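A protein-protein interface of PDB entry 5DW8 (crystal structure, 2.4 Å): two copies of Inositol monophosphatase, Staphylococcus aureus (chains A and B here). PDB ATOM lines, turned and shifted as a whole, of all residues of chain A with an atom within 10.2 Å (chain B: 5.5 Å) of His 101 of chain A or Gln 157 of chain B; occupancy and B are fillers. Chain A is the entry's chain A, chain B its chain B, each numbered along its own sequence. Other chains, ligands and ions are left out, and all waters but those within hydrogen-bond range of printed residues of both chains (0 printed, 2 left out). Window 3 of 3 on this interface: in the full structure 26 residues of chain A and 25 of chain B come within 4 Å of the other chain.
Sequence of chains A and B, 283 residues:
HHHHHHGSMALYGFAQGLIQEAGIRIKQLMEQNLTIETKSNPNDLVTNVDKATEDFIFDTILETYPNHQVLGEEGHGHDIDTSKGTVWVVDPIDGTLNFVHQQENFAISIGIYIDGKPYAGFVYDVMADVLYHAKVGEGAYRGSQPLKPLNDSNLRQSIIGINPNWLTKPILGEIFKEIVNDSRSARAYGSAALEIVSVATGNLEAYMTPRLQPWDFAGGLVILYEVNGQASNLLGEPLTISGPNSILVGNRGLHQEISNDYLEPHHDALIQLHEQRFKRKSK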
ATOM      1  N   MET A  30      13.399 -26.511 -36.682  1.00  0.00           N
ATOM      2  CA  MET A  30      13.773 -25.692 -35.529  1.00  0.00           C
ATOM      3  C   MET A  30      13.118 -24.336 -35.620  1.00  0.00           C
ATOM      4  O   MET A  30      12.536 -23.873 -34.654  1.00  0.00           O
ATOM      5  CB  MET A  30      15.286 -25.493 -35.437  1.00  0.00           C
ATOM      6  CG  MET A  30      16.071 -26.741 -35.078  1.00  0.00           C
ATOM      7  SD  MET A  30      17.812 -26.439 -35.427  1.00  0.00           S
ATOM      8  CE  MET A  30      18.248 -25.364 -34.063  1.00  0.00           C
ATOM      9  N   ASN A  43      11.412 -31.107 -23.733  1.00  0.00           N
ATOM     10  CA  ASN A  43      12.353 -31.582 -24.766  1.00  0.00           C
ATOM     11  C   ASN A  43      11.713 -32.645 -25.679  1.00  0.00           C
ATOM     12  O   ASN A  43      12.323 -33.667 -26.026  1.00  0.00           O
ATOM     13  CB  ASN A  43      13.690 -32.057 -24.148  1.00  0.00           C
ATOM     14  CG  ASN A  43      13.515 -32.819 -22.836  1.00  0.00           C
ATOM     15  OD1 ASN A  43      13.817 -34.004 -22.756  1.00  0.00           O
ATOM     16  ND2 ASN A  43      13.046 -32.133 -21.797  1.00  0.00           N
ATOM     17  N   LEU A  45      10.633 -31.558 -28.613  1.00  0.00           N
ATOM     18  CA  LEU A  45      11.108 -31.133 -29.909  1.00  0.00           C
ATOM     19  C   LEU A  45      12.182 -32.086 -30.396  1.00  0.00           C
ATOM     20  O   LEU A  45      12.104 -32.582 -31.512  1.00  0.00           O
ATOM     21  CB  LEU A  45      11.692 -29.717 -29.867  1.00  0.00           C
ATOM     22  CG  LEU A  45      12.499 -29.356 -31.139  1.00  0.00           C
ATOM     23  CD1 LEU A  45      11.649 -29.509 -32.392  1.00  0.00           C
ATOM     24  CD2 LEU A  45      13.075 -27.953 -31.073  1.00  0.00           C
ATOM     25  N   VAL A  46      13.186 -32.323 -29.561  1.00  0.00           N
ATOM     26  CA  VAL A  46      14.368 -33.066 -29.989  1.00  0.00           C
ATOM     27  C   VAL A  46      14.032 -34.495 -30.377  1.00  0.00           C
ATOM     28  O   VAL A  46      14.695 -35.054 -31.244  1.00  0.00           O
ATOM     29  CB  VAL A  46      15.526 -33.026 -28.933  1.00  0.00           C
ATOM     30  CG1 VAL A  46      15.085 -33.543 -27.566  1.00  0.00           C
ATOM     31  CG2 VAL A  46      16.768 -33.771 -29.430  1.00  0.00           C
ATOM     32  N   ILE A  93      21.011 -37.049 -35.123  1.00  0.00           N
ATOM     33  CA  ILE A  93      21.562 -35.978 -34.284  1.00  0.00           C
ATOM     34  C   ILE A  93      22.567 -36.468 -33.214  1.00  0.00           C
ATOM     35  O   ILE A  93      22.183 -36.979 -32.154  1.00  0.00           O
ATOM     36  CB  ILE A  93      20.457 -35.135 -33.611  1.00  0.00           C
ATOM     37  CG1 ILE A  93      19.627 -34.397 -34.667  1.00  0.00           C
ATOM     38  CG2 ILE A  93      21.054 -34.087 -32.669  1.00  0.00           C
ATOM     39  CD1 ILE A  93      18.316 -35.059 -34.991  1.00  0.00           C
ATOM     40  N   GLY A  95      24.754 -35.152 -30.442  1.00  0.00           N
ATOM     41  CA  GLY A  95      24.740 -33.970 -29.565  1.00  0.00           C
ATOM     42  C   GLY A  95      23.324 -33.480 -29.306  1.00  0.00           C
ATOM     43  O   GLY A  95      23.026 -32.322 -29.517  1.00  0.00           O
ATOM     44  N   THR A  96      22.450 -34.359 -28.825  1.00  0.00           N
ATOM     45  CA  THR A  96      21.037 -34.000 -28.561  1.00  0.00           C
ATOM     46  C   THR A  96      20.934 -32.931 -27.513  1.00  0.00           C
ATOM     47  O   THR A  96      20.163 -31.984 -27.668  1.00  0.00           O
ATOM     48  CB  THR A  96      20.120 -35.188 -28.103  1.00  0.00           C
ATOM     49  OG1 THR A  96      20.666 -35.858 -26.947  1.00  0.00           O
ATOM     50  CG2 THR A  96      19.922 -36.183 -29.216  1.00  0.00           C
ATOM     51  N   LEU A  97      21.695 -33.074 -26.437  1.00  0.00           N
ATOM     52  CA  LEU A  97      21.662 -32.051 -25.428  1.00  0.00           C
ATOM     53  C   LEU A  97      22.061 -30.722 -26.002  1.00  0.00           C
ATOM     54  O   LEU A  97      21.355 -29.753 -25.786  1.00  0.00           O
ATOM     55  CB  LEU A  97      22.532 -32.399 -24.241  1.00  0.00           C
ATOM     56  CG  LEU A  97      21.992 -33.568 -23.440  1.00  0.00           C
ATOM     57  CD1 LEU A  97      22.976 -33.835 -22.338  1.00  0.00           C
ATOM     58  CD2 LEU A  97      20.591 -33.368 -22.872  1.00  0.00           C
ATOM     59  N   ASN A  98      23.162 -30.665 -26.750  1.00  0.00           N
ATOM     60  CA  ASN A  98      23.609 -29.413 -27.355  1.00  0.00           C
ATOM     61  C   ASN A  98      22.499 -28.893 -28.247  1.00  0.00           C
ATOM     62  O   ASN A  98      22.187 -27.706 -28.241  1.00  0.00           O
ATOM     63  CB  ASN A  98      24.868 -29.608 -28.226  1.00  0.00           C
ATOM     64  CG  ASN A  98      26.146 -29.894 -27.425  1.00  0.00           C
ATOM     65  OD1 ASN A  98      26.218 -29.761 -26.198  1.00  0.00           O
ATOM     66  ND2 ASN A  98      27.175 -30.296 -28.147  1.00  0.00           N
ATOM     67  N   PHE A  99      21.898 -29.786 -29.026  1.00  0.00           N
ATOM     68  CA  PHE A  99      20.784 -29.405 -29.913  1.00  0.00           C
ATOM     69  C   PHE A  99      19.668 -28.672 -29.138  1.00  0.00           C
ATOM     70  O   PHE A  99      19.233 -27.603 -29.542  1.00  0.00           O
ATOM     71  CB  PHE A  99      20.212 -30.642 -30.661  1.00  0.00           C
ATOM     72  CG  PHE A  99      18.900 -30.366 -31.344  1.00  0.00           C
ATOM     73  CD1 PHE A  99      18.865 -29.937 -32.653  1.00  0.00           C
ATOM     74  CD2 PHE A  99      17.710 -30.490 -30.653  1.00  0.00           C
ATOM     75  CE1 PHE A  99      17.667 -29.650 -33.267  1.00  0.00           C
ATOM     76  CE2 PHE A  99      16.513 -30.199 -31.250  1.00  0.00           C
ATOM     77  CZ  PHE A  99      16.482 -29.767 -32.553  1.00  0.00           C
ATOM     78  N   VAL A 100      19.228 -29.287 -28.035  1.00  0.00           N
ATOM     79  CA  VAL A 100      18.187 -28.762 -27.127  1.00  0.00           C
ATOM     80  C   VAL A 100      18.559 -27.503 -26.333  1.00  0.00           C
ATOM     81  O   VAL A 100      17.704 -26.661 -26.123  1.00  0.00           O
ATOM     82  CB  VAL A 100      17.781 -29.844 -26.073  1.00  0.00           C
ATOM     83  CG1 VAL A 100      17.001 -29.257 -24.898  1.00  0.00           C
ATOM     84  CG2 VAL A 100      16.973 -30.947 -26.711  1.00  0.00           C
ATOM     85  N   HIS A 101      19.791 -27.417 -25.824  1.00  0.00           N
ATOM     86  CA  HIS A 101      20.225 -26.290 -24.941  1.00  0.00           C
ATOM     87  C   HIS A 101      20.977 -25.171 -25.661  1.00  0.00           C
ATOM     88  O   HIS A 101      20.974 -24.010 -25.223  1.00  0.00           O
ATOM     89  CB  HIS A 101      21.101 -26.819 -23.808  1.00  0.00           C
ATOM     90  CG  HIS A 101      20.403 -27.818 -22.933  1.00  0.00           C
ATOM     91  ND1 HIS A 101      19.747 -27.456 -21.774  1.00  0.00           N
ATOM     92  CD2 HIS A 101      20.237 -29.157 -23.059  1.00  0.00           C
ATOM     93  CE1 HIS A 101      19.205 -28.531 -21.228  1.00  0.00           C
ATOM     94  NE2 HIS A 101      19.488 -29.574 -21.989  1.00  0.00           N
ATOM     95  N   GLN A 102      21.644 -25.531 -26.749  1.00  0.00           N
ATOM     96  CA  GLN A 102      22.469 -24.601 -27.507  1.00  0.00           C
ATOM     97  C   GLN A 102      21.908 -24.316 -28.919  1.00  0.00           C
ATOM     98  O   GLN A 102      22.235 -23.301 -29.514  1.00  0.00           O
ATOM     99  CB  GLN A 102      23.892 -25.171 -27.632  1.00  0.00           C
ATOM    100  CG  GLN A 102      24.470 -25.744 -26.341  1.00  0.00           C
ATOM    101  CD  GLN A 102      25.980 -25.959 -26.428  1.00  0.00           C
ATOM    102  OE1 GLN A 102      26.475 -26.475 -27.430  1.00  0.00           O
ATOM    103  NE2 GLN A 102      26.717 -25.557 -25.394  1.00  0.00           N
ATOM    104  N   GLN A 103      21.107 -25.235 -29.464  1.00  0.00           N
ATOM    105  CA  GLN A 103      20.583 -25.113 -30.802  1.00  0.00           C
ATOM    106  C   GLN A 103      21.742 -24.960 -31.789  1.00  0.00           C
ATOM    107  O   GLN A 103      21.645 -24.222 -32.781  1.00  0.00           O
ATOM    108  CB  GLN A 103      19.611 -23.926 -30.909  1.00  0.00           C
ATOM    109  CG  GLN A 103      18.465 -23.932 -29.904  1.00  0.00           C
ATOM    110  CD  GLN A 103      18.797 -23.214 -28.596  1.00  0.00           C
ATOM    111  OE1 GLN A 103      19.364 -22.109 -28.591  1.00  0.00           O
ATOM    112  NE2 GLN A 103      18.440 -23.844 -27.470  1.00  0.00           N
ATOM    113  N   GLU A 104      22.838 -25.648 -31.486  1.00  0.00           N
ATOM    114  CA  GLU A 104      24.025 -25.670 -32.322  1.00  0.00           C
ATOM    115  C   GLU A 104      25.003 -26.719 -31.778  1.00  0.00           C
ATOM    116  O   GLU A 104      24.676 -27.428 -30.853  1.00  0.00           O
ATOM    117  CB  GLU A 104      24.672 -24.288 -32.373  1.00  0.00           C
ATOM    118  CG  GLU A 104      25.700 -23.996 -31.283  1.00  0.00           C
ATOM    119  CD  GLU A 104      26.061 -22.536 -31.222  1.00  0.00           C
ATOM    120  OE1 GLU A 104      26.617 -22.093 -30.201  1.00  0.00           O
ATOM    121  OE2 GLU A 104      25.780 -21.833 -32.195  1.00  0.00           O
ATOM    122  N   ASN A 105      26.194 -26.810 -32.357  1.00  0.00           N
ATOM    123  CA  ASN A 105      27.162 -27.874 -32.034  1.00  0.00           C
ATOM    124  C   ASN A 105      26.603 -29.299 -32.055  1.00  0.00           C
ATOM    125  O   ASN A 105      26.914 -30.094 -31.168  1.00  0.00           O
ATOM    126  CB  ASN A 105      27.823 -27.591 -30.682  1.00  0.00           C
ATOM    127  CG  ASN A 105      28.397 -26.185 -30.612  1.00  0.00           C
ATOM    128  OD1 ASN A 105      29.061 -25.743 -31.536  1.00  0.00           O
ATOM    129  ND2 ASN A 105      28.097 -25.463 -29.535  1.00  0.00           N
ATOM    130  N   PHE A 106      25.777 -29.620 -33.048  1.00  0.00           N
ATOM    131  CA  PHE A 106      25.333 -30.989 -33.262  1.00  0.00           C
ATOM    132  C   PHE A 106      25.555 -31.397 -34.738  1.00  0.00           C
ATOM    133  O   PHE A 106      25.775 -30.546 -35.609  1.00  0.00           O
ATOM    134  CB  PHE A 106      23.858 -31.134 -32.851  1.00  0.00           C
ATOM    135  CG  PHE A 106      22.928 -30.259 -33.630  1.00  0.00           C
ATOM    136  CD1 PHE A 106      22.408 -30.688 -34.860  1.00  0.00           C
ATOM    137  CD2 PHE A 106      22.588 -28.988 -33.164  1.00  0.00           C
ATOM    138  CE1 PHE A 106      21.573 -29.864 -35.607  1.00  0.00           C
ATOM    139  CE2 PHE A 106      21.734 -28.164 -33.896  1.00  0.00           C
ATOM    140  CZ  PHE A 106      21.228 -28.601 -35.117  1.00  0.00           C
ATOM    141  N   TYR A 189      33.184 -31.003 -25.886  1.00  0.00           N
ATOM    142  CA  TYR A 189      32.237 -30.304 -26.765  1.00  0.00           C
ATOM    143  C   TYR A 189      30.837 -30.929 -26.824  1.00  0.00           C
ATOM    144  O   TYR A 189      29.898 -30.272 -27.261  1.00  0.00           O
ATOM    145  CB  TYR A 189      32.823 -30.122 -28.176  1.00  0.00           C
ATOM    146  CG  TYR A 189      34.081 -29.326 -28.178  1.00  0.00           C
ATOM    147  CD1 TYR A 189      34.112 -28.048 -27.648  1.00  0.00           C
ATOM    148  CD2 TYR A 189      35.252 -29.824 -28.741  1.00  0.00           C
ATOM    149  CE1 TYR A 189      35.264 -27.293 -27.674  1.00  0.00           C
ATOM    150  CE2 TYR A 189      36.422 -29.073 -28.769  1.00  0.00           C
ATOM    151  CZ  TYR A 189      36.427 -27.817 -28.214  1.00  0.00           C
ATOM    152  OH  TYR A 189      37.579 -27.046 -28.236  1.00  0.00           O
ATOM    153  N   GLY A 190      30.695 -32.181 -26.398  1.00  0.00           N
ATOM    154  CA  GLY A 190      29.377 -32.817 -26.281  1.00  0.00           C
ATOM    155  C   GLY A 190      28.843 -33.457 -27.555  1.00  0.00           C
ATOM    156  O   GLY A 190      27.664 -33.733 -27.651  1.00  0.00           O
ATOM    157  N   SER B 153      17.033 -21.919 -14.507  1.00  0.00           N
ATOM    158  CA  SER B 153      17.012 -23.348 -14.695  1.00  0.00           C
ATOM    159  C   SER B 153      17.435 -23.997 -13.364  1.00  0.00           C
ATOM    160  O   SER B 153      18.142 -23.385 -12.567  1.00  0.00           O
ATOM    161  CB  SER B 153      17.971 -23.692 -15.821  1.00  0.00           C
ATOM    162  OG  SER B 153      19.307 -23.470 -15.417  1.00  0.00           O
ATOM    163  N   ASN B 154      16.976 -25.221 -13.095  1.00  0.00           N
ATOM    164  CA  ASN B 154      17.580 -25.988 -11.997  1.00  0.00           C
ATOM    165  C   ASN B 154      18.842 -26.614 -12.513  1.00  0.00           C
ATOM    166  O   ASN B 154      19.053 -26.690 -13.737  1.00  0.00           O
ATOM    167  CB  ASN B 154      16.733 -27.141 -11.473  1.00  0.00           C
ATOM    168  CG  ASN B 154      15.312 -27.043 -11.836  1.00  0.00           C
ATOM    169  OD1 ASN B 154      14.595 -26.202 -11.315  1.00  0.00           O
ATOM    170  ND2 ASN B 154      14.865 -27.952 -12.708  1.00  0.00           N
ATOM    171  N   LEU B 155      19.636 -27.140 -11.582  1.00  0.00           N
ATOM    172  CA  LEU B 155      20.884 -27.777 -11.943  1.00  0.00           C
ATOM    173  C   LEU B 155      20.619 -29.014 -12.818  1.00  0.00           C
ATOM    174  O   LEU B 155      21.303 -29.218 -13.841  1.00  0.00           O
ATOM    175  CB  LEU B 155      21.684 -28.120 -10.704  1.00  0.00           C
ATOM    176  CG  LEU B 155      23.063 -28.688 -10.998  1.00  0.00           C
ATOM    177  CD1 LEU B 155      23.868 -27.795 -11.944  1.00  0.00           C
ATOM    178  CD2 LEU B 155      23.820 -28.956  -9.709  1.00  0.00           C
ATOM    179  N   ARG B 156      19.575 -29.769 -12.461  1.00  0.00           N
ATOM    180  CA  ARG B 156      19.208 -30.973 -13.180  1.00  0.00           C
ATOM    181  C   ARG B 156      18.969 -30.888 -14.673  1.00  0.00           C
ATOM    182  O   ARG B 156      19.077 -31.887 -15.346  1.00  0.00           O
ATOM    183  CB  ARG B 156      17.945 -31.561 -12.560  1.00  0.00           C
ATOM    184  CG  ARG B 156      18.285 -32.767 -11.744  1.00  0.00           C
ATOM    185  CD  ARG B 156      17.214 -33.140 -10.761  1.00  0.00           C
ATOM    186  NE  ARG B 156      17.792 -34.116  -9.824  1.00  0.00           N
ATOM    187  CZ  ARG B 156      18.377 -33.811  -8.665  1.00  0.00           C
ATOM    188  NH1 ARG B 156      18.464 -32.539  -8.221  1.00  0.00           N
ATOM    189  NH2 ARG B 156      18.842 -34.804  -7.920  1.00  0.00           N
ATOM    190  N   GLN B 157      18.569 -29.733 -15.190  1.00  0.00           N
ATOM    191  CA  GLN B 157      18.381 -29.603 -16.655  1.00  0.00           C
ATOM    192  C   GLN B 157      19.389 -28.672 -17.261  1.00  0.00           C
ATOM    193  O   GLN B 157      19.143 -28.137 -18.325  1.00  0.00           O
ATOM    194  CB  GLN B 157      16.966 -29.105 -17.026  1.00  0.00           C
ATOM    195  CG  GLN B 157      15.856 -30.141 -16.828  1.00  0.00           C
ATOM    196  CD  GLN B 157      15.049 -29.907 -15.539  1.00  0.00           C
ATOM    197  OE1 GLN B 157      14.529 -28.795 -15.293  1.00  0.00           O
ATOM    198  NE2 GLN B 157      14.908 -30.965 -14.726  1.00  0.00           N
ATOM    199  N   SER B 158      20.518 -28.485 -16.594  1.00  0.00           N
ATOM    200  CA  SER B 158      21.466 -27.427 -16.947  1.00  0.00           C
ATOM    201  C   SER B 158      22.782 -28.035 -17.462  1.00  0.00           C
ATOM    202  O   SER B 158      23.231 -29.089 -17.004  1.00  0.00           O
ATOM    203  CB  SER B 158      21.746 -26.506 -15.730  1.00  0.00           C
ATOM    204  OG  SER B 158      20.557 -25.870 -15.229  1.00  0.00           O
ATOM    205  N   ILE B 159      23.385 -27.374 -18.439  1.00  0.00           N
ATOM    206  CA  ILE B 159      24.709 -27.758 -18.902  1.00  0.00           C
ATOM    207  C   ILE B 159      25.664 -26.785 -18.263  1.00  0.00           C
ATOM    208  O   ILE B 159      25.422 -25.597 -18.254  1.00  0.00           O
ATOM    209  CB  ILE B 159      24.841 -27.722 -20.458  1.00  0.00           C
ATOM    210  CG1 ILE B 159      23.635 -28.392 -21.098  1.00  0.00           C
ATOM    211  CG2 ILE B 159      26.127 -28.416 -20.890  1.00  0.00           C
ATOM    212  CD1 ILE B 159      23.915 -29.096 -22.384  1.00  0.00           C
ATOM    213  N   ARG B 184      22.747 -31.872 -16.112  1.00  0.00           N
ATOM    214  CA  ARG B 184      22.465 -32.693 -17.312  1.00  0.00           C
ATOM    215  C   ARG B 184      23.738 -33.153 -18.062  1.00  0.00           C
ATOM    216  O   ARG B 184      23.838 -34.268 -18.476  1.00  0.00           O
ATOM    217  CB  ARG B 184      21.520 -31.930 -18.242  1.00  0.00           C
ATOM    218  CG  ARG B 184      21.203 -32.604 -19.557  1.00  0.00           C
ATOM    219  CD  ARG B 184      20.374 -33.878 -19.399  1.00  0.00           C
ATOM    220  NE  ARG B 184      19.143 -33.602 -18.681  1.00  0.00           N
ATOM    221  CZ  ARG B 184      18.797 -34.138 -17.515  1.00  0.00           C
ATOM    222  NH1 ARG B 184      19.587 -35.039 -16.920  1.00  0.00           N
ATOM    223  NH2 ARG B 184      17.639 -33.792 -16.948  1.00  0.00           N
ATOM    224  N   GLY B 202      22.816 -17.892 -22.919  1.00  0.00           N
ATOM    225  CA  GLY B 202      22.017 -19.113 -22.671  1.00  0.00           C
ATOM    226  C   GLY B 202      22.623 -20.379 -23.251  1.00  0.00           C
ATOM    227  O   GLY B 202      22.036 -21.464 -23.182  1.00  0.00           O
ATOM    228  N   ASN B 203      23.815 -20.262 -23.804  1.00  0.00           N
ATOM    229  CA  ASN B 203      24.500 -21.416 -24.360  1.00  0.00           C
ATOM    230  C   ASN B 203      25.008 -22.411 -23.289  1.00  0.00           C
ATOM    231  O   ASN B 203      25.072 -23.613 -23.574  1.00  0.00           O
ATOM    232  CB  ASN B 203      25.652 -20.962 -25.242  1.00  0.00           C
ATOM    233  CG  ASN B 203      25.682 -21.674 -26.580  1.00  0.00           C
ATOM    234  OD1 ASN B 203      24.865 -21.374 -27.476  1.00  0.00           O
ATOM    235  ND2 ASN B 203      26.633 -22.622 -26.733  1.00  0.00           N
ATOM    236  N   GLU B 205      24.262 -22.828 -18.899  1.00  0.00           N
ATOM    237  CA  GLU B 205      23.518 -22.237 -17.780  1.00  0.00           C
ATOM    238  C   GLU B 205      24.460 -21.786 -16.653  1.00  0.00           C
ATOM    239  O   GLU B 205      24.145 -20.866 -15.888  1.00  0.00           O
ATOM    240  CB  GLU B 205      22.403 -23.178 -17.264  1.00  0.00           C
ATOM    241  CG  GLU B 205      21.276 -23.398 -18.259  1.00  0.00           C
ATOM    242  CD  GLU B 205      21.659 -24.305 -19.424  1.00  0.00           C
ATOM    243  OE1 GLU B 205      22.205 -25.397 -19.199  1.00  0.00           O
ATOM    244  OE2 GLU B 205      21.396 -23.956 -20.579  1.00  0.00           O
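NE2 of Gln 102 of chain A sits at hydrogen-bond distance from O of Asn 203 of chain B (3.1 Å).
OE1 of Glu 104 of chain A sits close to OD1 of Asn 203 of chain B, at 3.3 Å.
The backbone carbonyl oxygen (O) of Gly 202 of chain B lies close to the backbone carbonyl oxygen (O) of His 101 of chain A (3.4 Å).
The side-chain amide nitrogen (NE2) of Gln 103 of chain A lies close to the backbone carbonyl oxygen (O) of His 101 of chain A, 3.4 Å away.
OE1 of Gln 102 of chain A lies within hydrogen-bond range of ND2 of Asn 105 of chain A, 2.8 Å away.
ND2 of Asn 154 of chain B lies within hydrogen-bond range of OE1 of Gln 157 of chain B, at 2.7 Å.
O of Arg 156 of chain B is in hydrogen-bond range of NH2 of Arg 184 of chain B, 2.9 Å away.
O of Ser 158 of chain B sits at hydrogen-bond distance from N of Arg 184 of chain B (3.0 Å).
The backbone NH (N) of Ile 159 of chain B sits at hydrogen-bond distance from the side-chain carboxylate (OE1) of Glu 205 of chain B.
Among the printed residues, pairs that only touch across the chains: Leu 97 of chain A with Arg 184 of chain B (3.5 Å), His 101 of chain A with Gln 157 of chain B (2.9 Å) and His 101 of chain A with Ile 159 of chain B (3.7 Å).
Printed residues of chain A within 4 Å of Gln 157 of chain B: His 101 (2.9 Å).
No residue of chain A comes within 4 Å of Asn 154 of chain B.
Asn 203 of chain B touches just these residues of chain A: Gln 102 (3.1 Å) and Glu 104 (3.3 Å).
Of the printed residues of chain B, Glu 104 of chain A touches Asn 203.
Of the printed residues of chain A, Arg 184 of chain B touches Leu 97.
Of the printed residues of chain B, Leu 97 of chain A touches Arg 184 (3.5 Å).
Of the printed residues of chain A, Gly 202 of chain B touches His 101.
Printed residues of chain A within 4 Å of Ile 159 of chain B: His 101 (3.7 Å).
Phe 99 of chain A touches none of the printed residues of chain B.
Asn 43 of chain A touches none of the printed residues of chain B.
The nearest residue of chain B that does not touch His 101 of chain A is Glu 205 of chain B (4.05 Å).
The nearest printed residue of chain B that does not touch Leu 97 of chain A is Ile 159 of chain B (4.03 Å).
Of the 19 printed residues of chain A, 4 touch a printed residue of chain B.
Of the 11 printed residues of chain B, 5 touch a printed residue of chain A.
No position is printed for both chains.
Of the 6 pairs that touch across the chains among the printed residues, none has its exchanged pair printed and touching as well.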
